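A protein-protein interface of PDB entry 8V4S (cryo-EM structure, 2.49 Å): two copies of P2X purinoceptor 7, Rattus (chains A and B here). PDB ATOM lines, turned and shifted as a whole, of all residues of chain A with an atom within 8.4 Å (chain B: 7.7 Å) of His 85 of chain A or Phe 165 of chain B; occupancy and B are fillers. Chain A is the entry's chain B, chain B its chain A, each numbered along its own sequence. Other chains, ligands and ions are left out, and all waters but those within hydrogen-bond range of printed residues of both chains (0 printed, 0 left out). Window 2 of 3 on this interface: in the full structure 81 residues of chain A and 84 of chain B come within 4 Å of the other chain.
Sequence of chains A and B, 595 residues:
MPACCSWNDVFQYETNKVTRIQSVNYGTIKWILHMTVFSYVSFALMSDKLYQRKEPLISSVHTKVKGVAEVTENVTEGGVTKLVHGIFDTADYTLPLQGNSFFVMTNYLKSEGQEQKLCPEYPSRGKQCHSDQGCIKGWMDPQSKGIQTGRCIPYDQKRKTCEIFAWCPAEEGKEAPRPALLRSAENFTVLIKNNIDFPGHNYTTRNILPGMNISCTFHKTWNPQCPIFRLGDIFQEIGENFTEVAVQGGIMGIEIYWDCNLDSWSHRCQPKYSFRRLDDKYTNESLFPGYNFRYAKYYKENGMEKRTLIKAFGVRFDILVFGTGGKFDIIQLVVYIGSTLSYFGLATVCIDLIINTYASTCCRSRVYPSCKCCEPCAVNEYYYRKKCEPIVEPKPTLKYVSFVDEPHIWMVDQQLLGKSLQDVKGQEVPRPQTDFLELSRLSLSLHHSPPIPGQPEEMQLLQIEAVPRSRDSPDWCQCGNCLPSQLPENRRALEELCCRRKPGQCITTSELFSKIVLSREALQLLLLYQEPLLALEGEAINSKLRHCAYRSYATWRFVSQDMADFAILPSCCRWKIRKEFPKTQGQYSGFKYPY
No position is printed for both chains.
Of the 10 pairs that touch across the chains among the printed residues, none has its exchanged pair printed and touching as well.
NE2 of Gln 116 of chain B sits at hydrogen-bond distance from OE1 of Glu 305 of chain B, at 3.3 Å.
The backbone NH of Val 71 of chain A lies within hydrogen-bond range of the backbone carbonyl oxygen of Gly 86 of chain A, 2.9 Å away.
O of Ile 147 of chain B is in hydrogen-bond range of N of Phe 165 of chain B (2.9 Å).
The side-chain sulfur (SG) of Cys 119 of chain B is disulfide-bonded to the side-chain sulfur (SG) of Cys 168 of chain B (2.0 Å).
The backbone carbonyl oxygen (O) of Ala 166 of chain B is in hydrogen-bond range of the backbone NH (N) of Lys 117 of chain B, at 2.8 Å.
Among the printed residues, pairs that only touch across the chains: His 85 of chain A with Phe 165 of chain B, Ile 87 of chain A with Phe 165 of chain B, Gly 86 of chain A with Gln 116 of chain B, Glu 70 of chain A with Ile 147 of chain B, Ile 87 of chain A with Trp 167 of chain B, Val 68 of chain A with Lys 145 of chain B, Ile 87 of chain A with Ile 147 of chain B, Ile 87 of chain A with Gly 146 of chain B and Ile 87 of chain A with Ala 166 of chain B.
Phe 165 of chain B touches just these residues of chain A: His 85 and Ile 87.
Printed residues of chain B within 4 Å of Val 68 of chain A: Lys 145 (3.7 Å).
Printed residues of chain A within 4 Å of Ile 147 of chain B: Glu 70 and Ile 87.
The nearest residue of chain B that does not touch His 85 of chain A is Gln 116 of chain B (4.4 Å).
The nearest residue of chain A that does not touch Phe 165 of chain B is Gly 86 of chain A (4.4 Å).
Hydrophobic or aromatic side chains of chain B within 4 Å of the printed part of chain A: Ile 147, Phe 165 and Trp 167.
Printed residues of chain A that touch a printed residue of chain B: Val 68, Glu 70, His 85, Gly 86 and Ile 87.
Among the printed residues, 10 pairs touch across the chains.
Among the printed residues, no Asp or Glu carboxylate lies within 4 Å of a Lys or Arg side-chain nitrogen of the other chain.
N of Ile 87 of chain A is in hydrogen-bond range of OE1 of Gln 116 of chain B, at 2.8 Å.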
ATOM      1  N   VAL A  68      11.476   1.110 -11.397  1.00  0.00           N
ATOM      2  CA  VAL A  68      11.472   1.558 -10.010  1.00  0.00           C
ATOM      3  C   VAL A  68      10.028   1.777  -9.586  1.00  0.00           C
ATOM      4  O   VAL A  68       9.169   2.078 -10.420  1.00  0.00           O
ATOM      5  CB  VAL A  68      12.301   2.846  -9.818  1.00  0.00           C
ATOM      6  CG1 VAL A  68      13.783   2.551  -9.951  1.00  0.00           C
ATOM      7  CG2 VAL A  68      11.886   3.900 -10.822  1.00  0.00           C
ATOM      8  N   ALA A  69       9.764   1.621  -8.293  1.00  0.00           N
ATOM      9  CA  ALA A  69       8.419   1.783  -7.757  1.00  0.00           C
ATOM     10  C   ALA A  69       8.459   2.679  -6.528  1.00  0.00           C
ATOM     11  O   ALA A  69       9.468   2.735  -5.827  1.00  0.00           O
ATOM     12  CB  ALA A  69       7.795   0.432  -7.397  1.00  0.00           C
ATOM     13  N   GLU A  70       7.362   3.384  -6.274  1.00  0.00           N
ATOM     14  CA  GLU A  70       7.226   4.212  -5.084  1.00  0.00           C
ATOM     15  C   GLU A  70       6.130   3.636  -4.197  1.00  0.00           C
ATOM     16  O   GLU A  70       5.031   3.338  -4.676  1.00  0.00           O
ATOM     17  CB  GLU A  70       6.913   5.662  -5.455  1.00  0.00           C
ATOM     18  CG  GLU A  70       5.913   5.814  -6.584  1.00  0.00           C
ATOM     19  CD  GLU A  70       5.650   7.264  -6.933  1.00  0.00           C
ATOM     20  OE1 GLU A  70       6.031   8.144  -6.134  1.00  0.00           O
ATOM     21  OE2 GLU A  70       5.067   7.525  -8.004  1.00  0.00           O
ATOM     22  N   VAL A  71       6.435   3.471  -2.911  1.00  0.00           N
ATOM     23  CA  VAL A  71       5.515   2.859  -1.958  1.00  0.00           C
ATOM     24  C   VAL A  71       5.383   3.771  -0.746  1.00  0.00           C
ATOM     25  O   VAL A  71       6.390   4.176  -0.154  1.00  0.00           O
ATOM     26  CB  VAL A  71       5.980   1.457  -1.533  1.00  0.00           C
ATOM     27  CG1 VAL A  71       5.049   0.890  -0.474  1.00  0.00           C
ATOM     28  CG2 VAL A  71       6.039   0.531  -2.736  1.00  0.00           C
ATOM     29  N   THR A  72       4.145   4.088  -0.377  1.00  0.00           N
ATOM     30  CA  THR A  72       3.881   4.827   0.845  1.00  0.00           C
ATOM     31  C   THR A  72       3.703   3.866   2.014  1.00  0.00           C
ATOM     32  O   THR A  72       3.207   2.747   1.854  1.00  0.00           O
ATOM     33  CB  THR A  72       2.633   5.697   0.694  1.00  0.00           C
ATOM     34  OG1 THR A  72       1.504   4.867   0.393  1.00  0.00           O
ATOM     35  CG2 THR A  72       2.821   6.709  -0.424  1.00  0.00           C
ATOM     36  N   GLU A  73       4.112   4.318   3.198  1.00  0.00           N
ATOM     37  CA  GLU A  73       4.047   3.520   4.422  1.00  0.00           C
ATOM     38  C   GLU A  73       4.803   2.203   4.269  1.00  0.00           C
ATOM     39  O   GLU A  73       5.588   1.823   5.136  1.00  0.00           O
ATOM     40  CB  GLU A  73       2.593   3.252   4.822  1.00  0.00           C
ATOM     41  N   LEU A  83       3.808   7.951   8.354  1.00  0.00           N
ATOM     42  CA  LEU A  83       3.814   7.657   6.926  1.00  0.00           C
ATOM     43  C   LEU A  83       5.206   7.841   6.330  1.00  0.00           C
ATOM     44  O   LEU A  83       5.749   8.947   6.330  1.00  0.00           O
ATOM     45  CB  LEU A  83       2.811   8.544   6.191  1.00  0.00           C
ATOM     46  CG  LEU A  83       2.770   8.377   4.672  1.00  0.00           C
ATOM     47  CD1 LEU A  83       2.342   6.967   4.295  1.00  0.00           C
ATOM     48  CD2 LEU A  83       1.850   9.409   4.036  1.00  0.00           C
ATOM     49  N   VAL A  84       5.777   6.754   5.818  1.00  0.00           N
ATOM     50  CA  VAL A  84       7.101   6.763   5.208  1.00  0.00           C
ATOM     51  C   VAL A  84       6.949   6.500   3.717  1.00  0.00           C
ATOM     52  O   VAL A  84       6.294   5.531   3.312  1.00  0.00           O
ATOM     53  CB  VAL A  84       8.033   5.728   5.863  1.00  0.00           C
ATOM     54  CG1 VAL A  84       8.631   6.290   7.143  1.00  0.00           C
ATOM     55  CG2 VAL A  84       7.280   4.439   6.149  1.00  0.00           C
ATOM     56  N   HIS A  85       7.546   7.366   2.906  1.00  0.00           N
ATOM     57  CA  HIS A  85       7.535   7.233   1.454  1.00  0.00           C
ATOM     58  C   HIS A  85       8.895   6.711   1.006  1.00  0.00           C
ATOM     59  O   HIS A  85       9.927   7.315   1.322  1.00  0.00           O
ATOM     60  CB  HIS A  85       7.223   8.575   0.793  1.00  0.00           C
ATOM     61  CG  HIS A  85       6.827   8.465  -0.646  1.00  0.00           C
ATOM     62  ND1 HIS A  85       7.730   8.181  -1.648  1.00  0.00           N
ATOM     63  CD2 HIS A  85       5.627   8.615  -1.253  1.00  0.00           C
ATOM     64  CE1 HIS A  85       7.101   8.153  -2.809  1.00  0.00           C
ATOM     65  NE2 HIS A  85       5.824   8.413  -2.599  1.00  0.00           N
ATOM     66  N   GLY A  86       8.898   5.590   0.278  1.00  0.00           N
ATOM     67  CA  GLY A  86      10.129   4.962  -0.138  1.00  0.00           C
ATOM     68  C   GLY A  86      10.096   4.599  -1.612  1.00  0.00           C
ATOM     69  O   GLY A  86       9.039   4.547  -2.241  1.00  0.00           O
ATOM     70  N   ILE A  87      11.288   4.350  -2.147  1.00  0.00           N
ATOM     71  CA  ILE A  87      11.462   3.962  -3.540  1.00  0.00           C
ATOM     72  C   ILE A  87      12.213   2.638  -3.585  1.00  0.00           C
ATOM     73  O   ILE A  87      13.124   2.387  -2.790  1.00  0.00           O
ATOM     74  CB  ILE A  87      12.190   5.061  -4.355  1.00  0.00           C
ATOM     75  CG1 ILE A  87      11.765   5.009  -5.823  1.00  0.00           C
ATOM     76  CG2 ILE A  87      13.704   4.963  -4.216  1.00  0.00           C
ATOM     77  CD1 ILE A  87      12.394   6.082  -6.677  1.00  0.00           C
ATOM     78  N   PHE A  88      11.779   1.759  -4.487  1.00  0.00           N
ATOM     79  CA  PHE A  88      12.411   0.462  -4.698  1.00  0.00           C
ATOM     80  C   PHE A  88      13.006   0.461  -6.099  1.00  0.00           C
ATOM     81  O   PHE A  88      12.299   0.733  -7.077  1.00  0.00           O
ATOM     82  CB  PHE A  88      11.436  -0.713  -4.529  1.00  0.00           C
ATOM     83  CG  PHE A  88      10.848  -0.867  -3.137  1.00  0.00           C
ATOM     84  CD1 PHE A  88       9.690  -0.187  -2.799  1.00  0.00           C
ATOM     85  CD2 PHE A  88      11.412  -1.703  -2.189  1.00  0.00           C
ATOM     86  CE1 PHE A  88       9.129  -0.319  -1.541  1.00  0.00           C
ATOM     87  CE2 PHE A  88      10.860  -1.832  -0.927  1.00  0.00           C
ATOM     88  CZ  PHE A  88       9.716  -1.142  -0.605  1.00  0.00           C
ATOM     89  N   GLU B 115      20.267   7.925   1.544  1.00  0.00           N
ATOM     90  CA  GLU B 115      18.959   8.096   2.157  1.00  0.00           C
ATOM     91  C   GLU B 115      17.934   8.402   1.073  1.00  0.00           C
ATOM     92  O   GLU B 115      18.251   9.033   0.064  1.00  0.00           O
ATOM     93  CB  GLU B 115      18.968   9.222   3.199  1.00  0.00           C
ATOM     94  CG  GLU B 115      19.784   8.916   4.441  1.00  0.00           C
ATOM     95  CD  GLU B 115      21.233   9.344   4.314  1.00  0.00           C
ATOM     96  OE1 GLU B 115      21.578   9.999   3.308  1.00  0.00           O
ATOM     97  OE2 GLU B 115      22.028   9.027   5.222  1.00  0.00           O
ATOM     98  N   GLN B 116      16.698   7.934   1.266  1.00  0.00           N
ATOM     99  CA  GLN B 116      15.637   8.159   0.244  1.00  0.00           C
ATOM    100  C   GLN B 116      15.154   9.609   0.339  1.00  0.00           C
ATOM    101  O   GLN B 116      14.366   9.903   1.259  1.00  0.00           O
ATOM    102  CB  GLN B 116      14.491   7.164   0.438  1.00  0.00           C
ATOM    103  CG  GLN B 116      14.903   5.723   0.187  1.00  0.00           C
ATOM    104  CD  GLN B 116      13.819   4.739   0.549  1.00  0.00           C
ATOM    105  OE1 GLN B 116      13.348   3.970  -0.284  1.00  0.00           O
ATOM    106  NE2 GLN B 116      13.419   4.751   1.811  1.00  0.00           N
ATOM    107  N   LYS B 117      15.605  10.473  -0.577  1.00  0.00           N
ATOM    108  CA  LYS B 117      15.250  11.916  -0.497  1.00  0.00           C
ATOM    109  C   LYS B 117      15.439  12.584  -1.863  1.00  0.00           C
ATOM    110  O   LYS B 117      15.919  11.906  -2.791  1.00  0.00           O
ATOM    111  CB  LYS B 117      16.126  12.601   0.556  1.00  0.00           C
ATOM    112  CG  LYS B 117      17.622  12.403   0.363  1.00  0.00           C
ATOM    113  CD  LYS B 117      18.442  12.759   1.583  1.00  0.00           C
ATOM    114  CE  LYS B 117      19.913  12.444   1.414  1.00  0.00           C
ATOM    115  NZ  LYS B 117      20.678  12.717   2.652  1.00  0.00           N
ATOM    116  N   LEU B 118      15.069  13.863  -1.974  1.00  0.00           N
ATOM    117  CA  LEU B 118      15.246  14.615  -3.247  1.00  0.00           C
ATOM    118  C   LEU B 118      16.727  14.961  -3.429  1.00  0.00           C
ATOM    119  O   LEU B 118      17.373  15.311  -2.423  1.00  0.00           O
ATOM    120  CB  LEU B 118      14.393  15.885  -3.199  1.00  0.00           C
ATOM    121  CG  LEU B 118      12.981  15.750  -3.765  1.00  0.00           C
ATOM    122  CD1 LEU B 118      12.285  17.101  -3.805  1.00  0.00           C
ATOM    123  CD2 LEU B 118      13.020  15.138  -5.154  1.00  0.00           C
ATOM    124  N   CYS B 119      17.229  14.877  -4.665  1.00  0.00           N
ATOM    125  CA  CYS B 119      18.649  15.216  -4.958  1.00  0.00           C
ATOM    126  C   CYS B 119      18.861  15.222  -6.476  1.00  0.00           C
ATOM    127  O   CYS B 119      18.110  14.516  -7.177  1.00  0.00           O
ATOM    128  CB  CYS B 119      19.596  14.209  -4.316  1.00  0.00           C
ATOM    129  SG  CYS B 119      19.294  12.492  -4.815  1.00  0.00           S
ATOM    130  N   PRO B 120      19.835  15.986  -7.020  1.00  0.00           N
ATOM    131  CA  PRO B 120      20.037  16.055  -8.472  1.00  0.00           C
ATOM    132  C   PRO B 120      20.649  14.769  -9.005  1.00  0.00           C
ATOM    133  O   PRO B 120      21.484  14.138  -8.353  1.00  0.00           O
ATOM    134  CB  PRO B 120      20.993  17.240  -8.637  1.00  0.00           C
ATOM    135  CG  PRO B 120      21.761  17.268  -7.363  1.00  0.00           C
ATOM    136  CD  PRO B 120      20.804  16.824  -6.286  1.00  0.00           C
ATOM    137  N   SER B 144      18.110   6.601 -14.217  1.00  0.00           N
ATOM    138  CA  SER B 144      18.621   7.223 -13.003  1.00  0.00           C
ATOM    139  C   SER B 144      18.083   6.576 -11.733  1.00  0.00           C
ATOM    140  O   SER B 144      18.545   6.924 -10.642  1.00  0.00           O
ATOM    141  CB  SER B 144      18.290   8.719 -12.991  1.00  0.00           C
ATOM    142  OG  SER B 144      16.890   8.935 -12.958  1.00  0.00           O
ATOM    143  N   LYS B 145      17.135   5.645 -11.856  1.00  0.00           N
ATOM    144  CA  LYS B 145      16.544   4.939 -10.719  1.00  0.00           C
ATOM    145  C   LYS B 145      15.927   5.922  -9.722  1.00  0.00           C
ATOM    146  O   LYS B 145      16.234   5.919  -8.529  1.00  0.00           O
ATOM    147  CB  LYS B 145      17.576   4.032 -10.042  1.00  0.00           C
ATOM    148  CG  LYS B 145      17.892   2.767 -10.819  1.00  0.00           C
ATOM    149  CD  LYS B 145      19.251   2.860 -11.489  1.00  0.00           C
ATOM    150  CE  LYS B 145      19.606   1.571 -12.207  1.00  0.00           C
ATOM    151  NZ  LYS B 145      20.999   1.596 -12.732  1.00  0.00           N
ATOM    152  N   GLY B 146      15.038   6.764 -10.238  1.00  0.00           N
ATOM    153  CA  GLY B 146      14.386   7.764  -9.414  1.00  0.00           C
ATOM    154  C   GLY B 146      13.190   8.346 -10.133  1.00  0.00           C
ATOM    155  O   GLY B 146      12.890   7.993 -11.276  1.00  0.00           O
ATOM    156  N   ILE B 147      12.503   9.247  -9.433  1.00  0.00           N
ATOM    157  CA  ILE B 147      11.307   9.908  -9.942  1.00  0.00           C
ATOM    158  C   ILE B 147      11.580  11.404  -9.994  1.00  0.00           C
ATOM    159  O   ILE B 147      11.846  12.027  -8.959  1.00  0.00           O
ATOM    160  CB  ILE B 147      10.075   9.604  -9.075  1.00  0.00           C
ATOM    161  CG1 ILE B 147      10.007   8.110  -8.757  1.00  0.00           C
ATOM    162  CG2 ILE B 147       8.806  10.066  -9.773  1.00  0.00           C
ATOM    163  CD1 ILE B 147       9.105   7.775  -7.596  1.00  0.00           C
ATOM    164  N   GLN B 148      11.502  11.977 -11.191  1.00  0.00           N
ATOM    165  CA  GLN B 148      11.774  13.398 -11.362  1.00  0.00           C
ATOM    166  C   GLN B 148      10.605  14.234 -10.857  1.00  0.00           C
ATOM    167  O   GLN B 148       9.439  13.925 -11.119  1.00  0.00           O
ATOM    168  CB  GLN B 148      12.044  13.711 -12.832  1.00  0.00           C
ATOM    169  CG  GLN B 148      13.244  12.986 -13.407  1.00  0.00           C
ATOM    170  CD  GLN B 148      13.446  13.276 -14.877  1.00  0.00           C
ATOM    171  OE1 GLN B 148      12.516  13.677 -15.573  1.00  0.00           O
ATOM    172  NE2 GLN B 148      14.666  13.069 -15.360  1.00  0.00           N
ATOM    173  N   THR B 149      10.922  15.304 -10.130  1.00  0.00           N
ATOM    174  CA  THR B 149       9.917  16.194  -9.568  1.00  0.00           C
ATOM    175  C   THR B 149       9.674  17.431 -10.424  1.00  0.00           C
ATOM    176  O   THR B 149       8.930  18.325 -10.008  1.00  0.00           O
ATOM    177  CB  THR B 149      10.311  16.614  -8.151  1.00  0.00           C
ATOM    178  OG1 THR B 149      11.667  17.080  -8.147  1.00  0.00           O
ATOM    179  CG2 THR B 149      10.179  15.440  -7.195  1.00  0.00           C
ATOM    180  N   CYS B 162      18.423  17.159 -13.659  1.00  0.00           N
ATOM    181  CA  CYS B 162      17.071  16.981 -13.149  1.00  0.00           C
ATOM    182  C   CYS B 162      17.093  16.530 -11.694  1.00  0.00           C
ATOM    183  O   CYS B 162      18.023  15.859 -11.236  1.00  0.00           O
ATOM    184  CB  CYS B 162      16.301  15.970 -13.997  1.00  0.00           C
ATOM    185  SG  CYS B 162      15.574  16.662 -15.498  1.00  0.00           S
ATOM    186  N   GLU B 163      16.050  16.910 -10.967  1.00  0.00           N
ATOM    187  CA  GLU B 163      15.932  16.633  -9.544  1.00  0.00           C
ATOM    188  C   GLU B 163      15.029  15.419  -9.355  1.00  0.00           C
ATOM    189  O   GLU B 163      13.866  15.439  -9.770  1.00  0.00           O
ATOM    190  CB  GLU B 163      15.372  17.853  -8.817  1.00  0.00           C
ATOM    191  CG  GLU B 163      15.243  17.675  -7.331  1.00  0.00           C
ATOM    192  CD  GLU B 163      14.314  18.688  -6.697  1.00  0.00           C
ATOM    193  OE1 GLU B 163      13.144  18.766  -7.126  1.00  0.00           O
ATOM    194  OE2 GLU B 163      14.746  19.392  -5.763  1.00  0.00           O
ATOM    195  N   ILE B 164      15.563  14.368  -8.733  1.00  0.00           N
ATOM    196  CA  ILE B 164      14.857  13.103  -8.582  1.00  0.00           C
ATOM    197  C   ILE B 164      14.743  12.758  -7.103  1.00  0.00           C
ATOM    198  O   ILE B 164      15.615  13.094  -6.293  1.00  0.00           O
ATOM    199  CB  ILE B 164      15.556  11.958  -9.347  1.00  0.00           C
ATOM    200  CG1 ILE B 164      16.956  11.711  -8.782  1.00  0.00           C
ATOM    201  CG2 ILE B 164      15.636  12.272 -10.830  1.00  0.00           C
ATOM    202  CD1 ILE B 164      17.694  10.576  -9.454  1.00  0.00           C
ATOM    203  N   PHE B 165      13.656  12.075  -6.755  1.00  0.00           N
ATOM    204  CA  PHE B 165      13.474  11.499  -5.427  1.00  0.00           C
ATOM    205  C   PHE B 165      13.923  10.043  -5.482  1.00  0.00           C
ATOM    206  O   PHE B 165      13.279   9.214  -6.132  1.00  0.00           O
ATOM    207  CB  PHE B 165      12.022  11.607  -4.969  1.00  0.00           C
ATOM    208  CG  PHE B 165      11.690  10.719  -3.805  1.00  0.00           C
ATOM    209  CD1 PHE B 165      12.104  11.049  -2.526  1.00  0.00           C
ATOM    210  CD2 PHE B 165      10.969   9.552  -3.990  1.00  0.00           C
ATOM    211  CE1 PHE B 165      11.805  10.231  -1.453  1.00  0.00           C
ATOM    212  CE2 PHE B 165      10.668   8.730  -2.921  1.00  0.00           C
ATOM    213  CZ  PHE B 165      11.086   9.071  -1.651  1.00  0.00           C
ATOM    214  N   ALA B 166      15.018   9.736  -4.802  1.00  0.00           N
ATOM    215  CA  ALA B 166      15.608   8.400  -4.833  1.00  0.00           C
ATOM    216  C   ALA B 166      16.619   8.313  -3.694  1.00  0.00           C
ATOM    217  O   ALA B 166      16.679   9.194  -2.830  1.00  0.00           O
ATOM    218  CB  ALA B 166      16.251   8.107  -6.189  1.00  0.00           C
ATOM    219  N   TRP B 167      17.407   7.242  -3.682  1.00  0.00           N
ATOM    220  CA  TRP B 167      18.521   7.165  -2.750  1.00  0.00           C
ATOM    221  C   TRP B 167      19.584   8.185  -3.141  1.00  0.00           C
ATOM    222  O   TRP B 167      19.958   8.294  -4.312  1.00  0.00           O
ATOM    223  CB  TRP B 167      19.113   5.759  -2.737  1.00  0.00           C
ATOM    224  CG  TRP B 167      18.165   4.704  -2.256  1.00  0.00           C
ATOM    225  CD1 TRP B 167      17.279   3.990  -3.011  1.00  0.00           C
ATOM    226  CD2 TRP B 167      18.012   4.237  -0.911  1.00  0.00           C
ATOM    227  NE1 TRP B 167      16.585   3.110  -2.220  1.00  0.00           N
ATOM    228  CE2 TRP B 167      17.015   3.241  -0.926  1.00  0.00           C
ATOM    229  CE3 TRP B 167      18.620   4.564   0.303  1.00  0.00           C
ATOM    230  CZ2 TRP B 167      16.614   2.571   0.226  1.00  0.00           C
ATOM    231  CZ3 TRP B 167      18.218   3.898   1.446  1.00  0.00           C
ATOM    232  CH2 TRP B 167      17.227   2.914   1.399  1.00  0.00           C
ATOM    233  N   CYS B 168      20.066   8.935  -2.157  1.00  0.00           N
ATOM    234  CA  CYS B 168      21.037   9.988  -2.385  1.00  0.00           C
ATOM    235  C   CYS B 168      22.200   9.835  -1.418  1.00  0.00           C
ATOM    236  O   CYS B 168      22.012   9.374  -0.286  1.00  0.00           O
ATOM    237  CB  CYS B 168      20.397  11.374  -2.213  1.00  0.00           C
ATOM    238  SG  CYS B 168      18.818  11.563  -3.070  1.00  0.00           S
ATOM    239  N   MET B 304      17.114   6.938  10.749  1.00  0.00           N
ATOM    240  CA  MET B 304      16.846   7.171   9.337  1.00  0.00           C
ATOM    241  C   MET B 304      17.391   6.000   8.537  1.00  0.00           C
ATOM    242  O   MET B 304      18.508   5.541   8.792  1.00  0.00           O
ATOM    243  CB  MET B 304      17.479   8.485   8.862  1.00  0.00           C
ATOM    244  CG  MET B 304      16.878   9.036   7.582  1.00  0.00           C
ATOM    245  SD  MET B 304      15.115   9.378   7.750  1.00  0.00           S
ATOM    246  CE  MET B 304      14.703   9.878   6.083  1.00  0.00           C
ATOM    247  N   GLU B 305      16.604   5.518   7.576  1.00  0.00           N
ATOM    248  CA  GLU B 305      17.009   4.378   6.764  1.00  0.00           C
ATOM    249  C   GLU B 305      18.186   4.739   5.870  1.00  0.00           C
ATOM    250  O   GLU B 305      18.067   5.592   4.986  1.00  0.00           O
ATOM    251  CB  GLU B 305      15.836   3.872   5.919  1.00  0.00           C
ATOM    252  CG  GLU B 305      14.583   3.561   6.718  1.00  0.00           C
ATOM    253  CD  GLU B 305      13.415   3.160   5.840  1.00  0.00           C
ATOM    254  OE1 GLU B 305      13.598   3.071   4.608  1.00  0.00           O
ATOM    255  OE2 GLU B 305      12.311   2.936   6.381  1.00  0.00           O
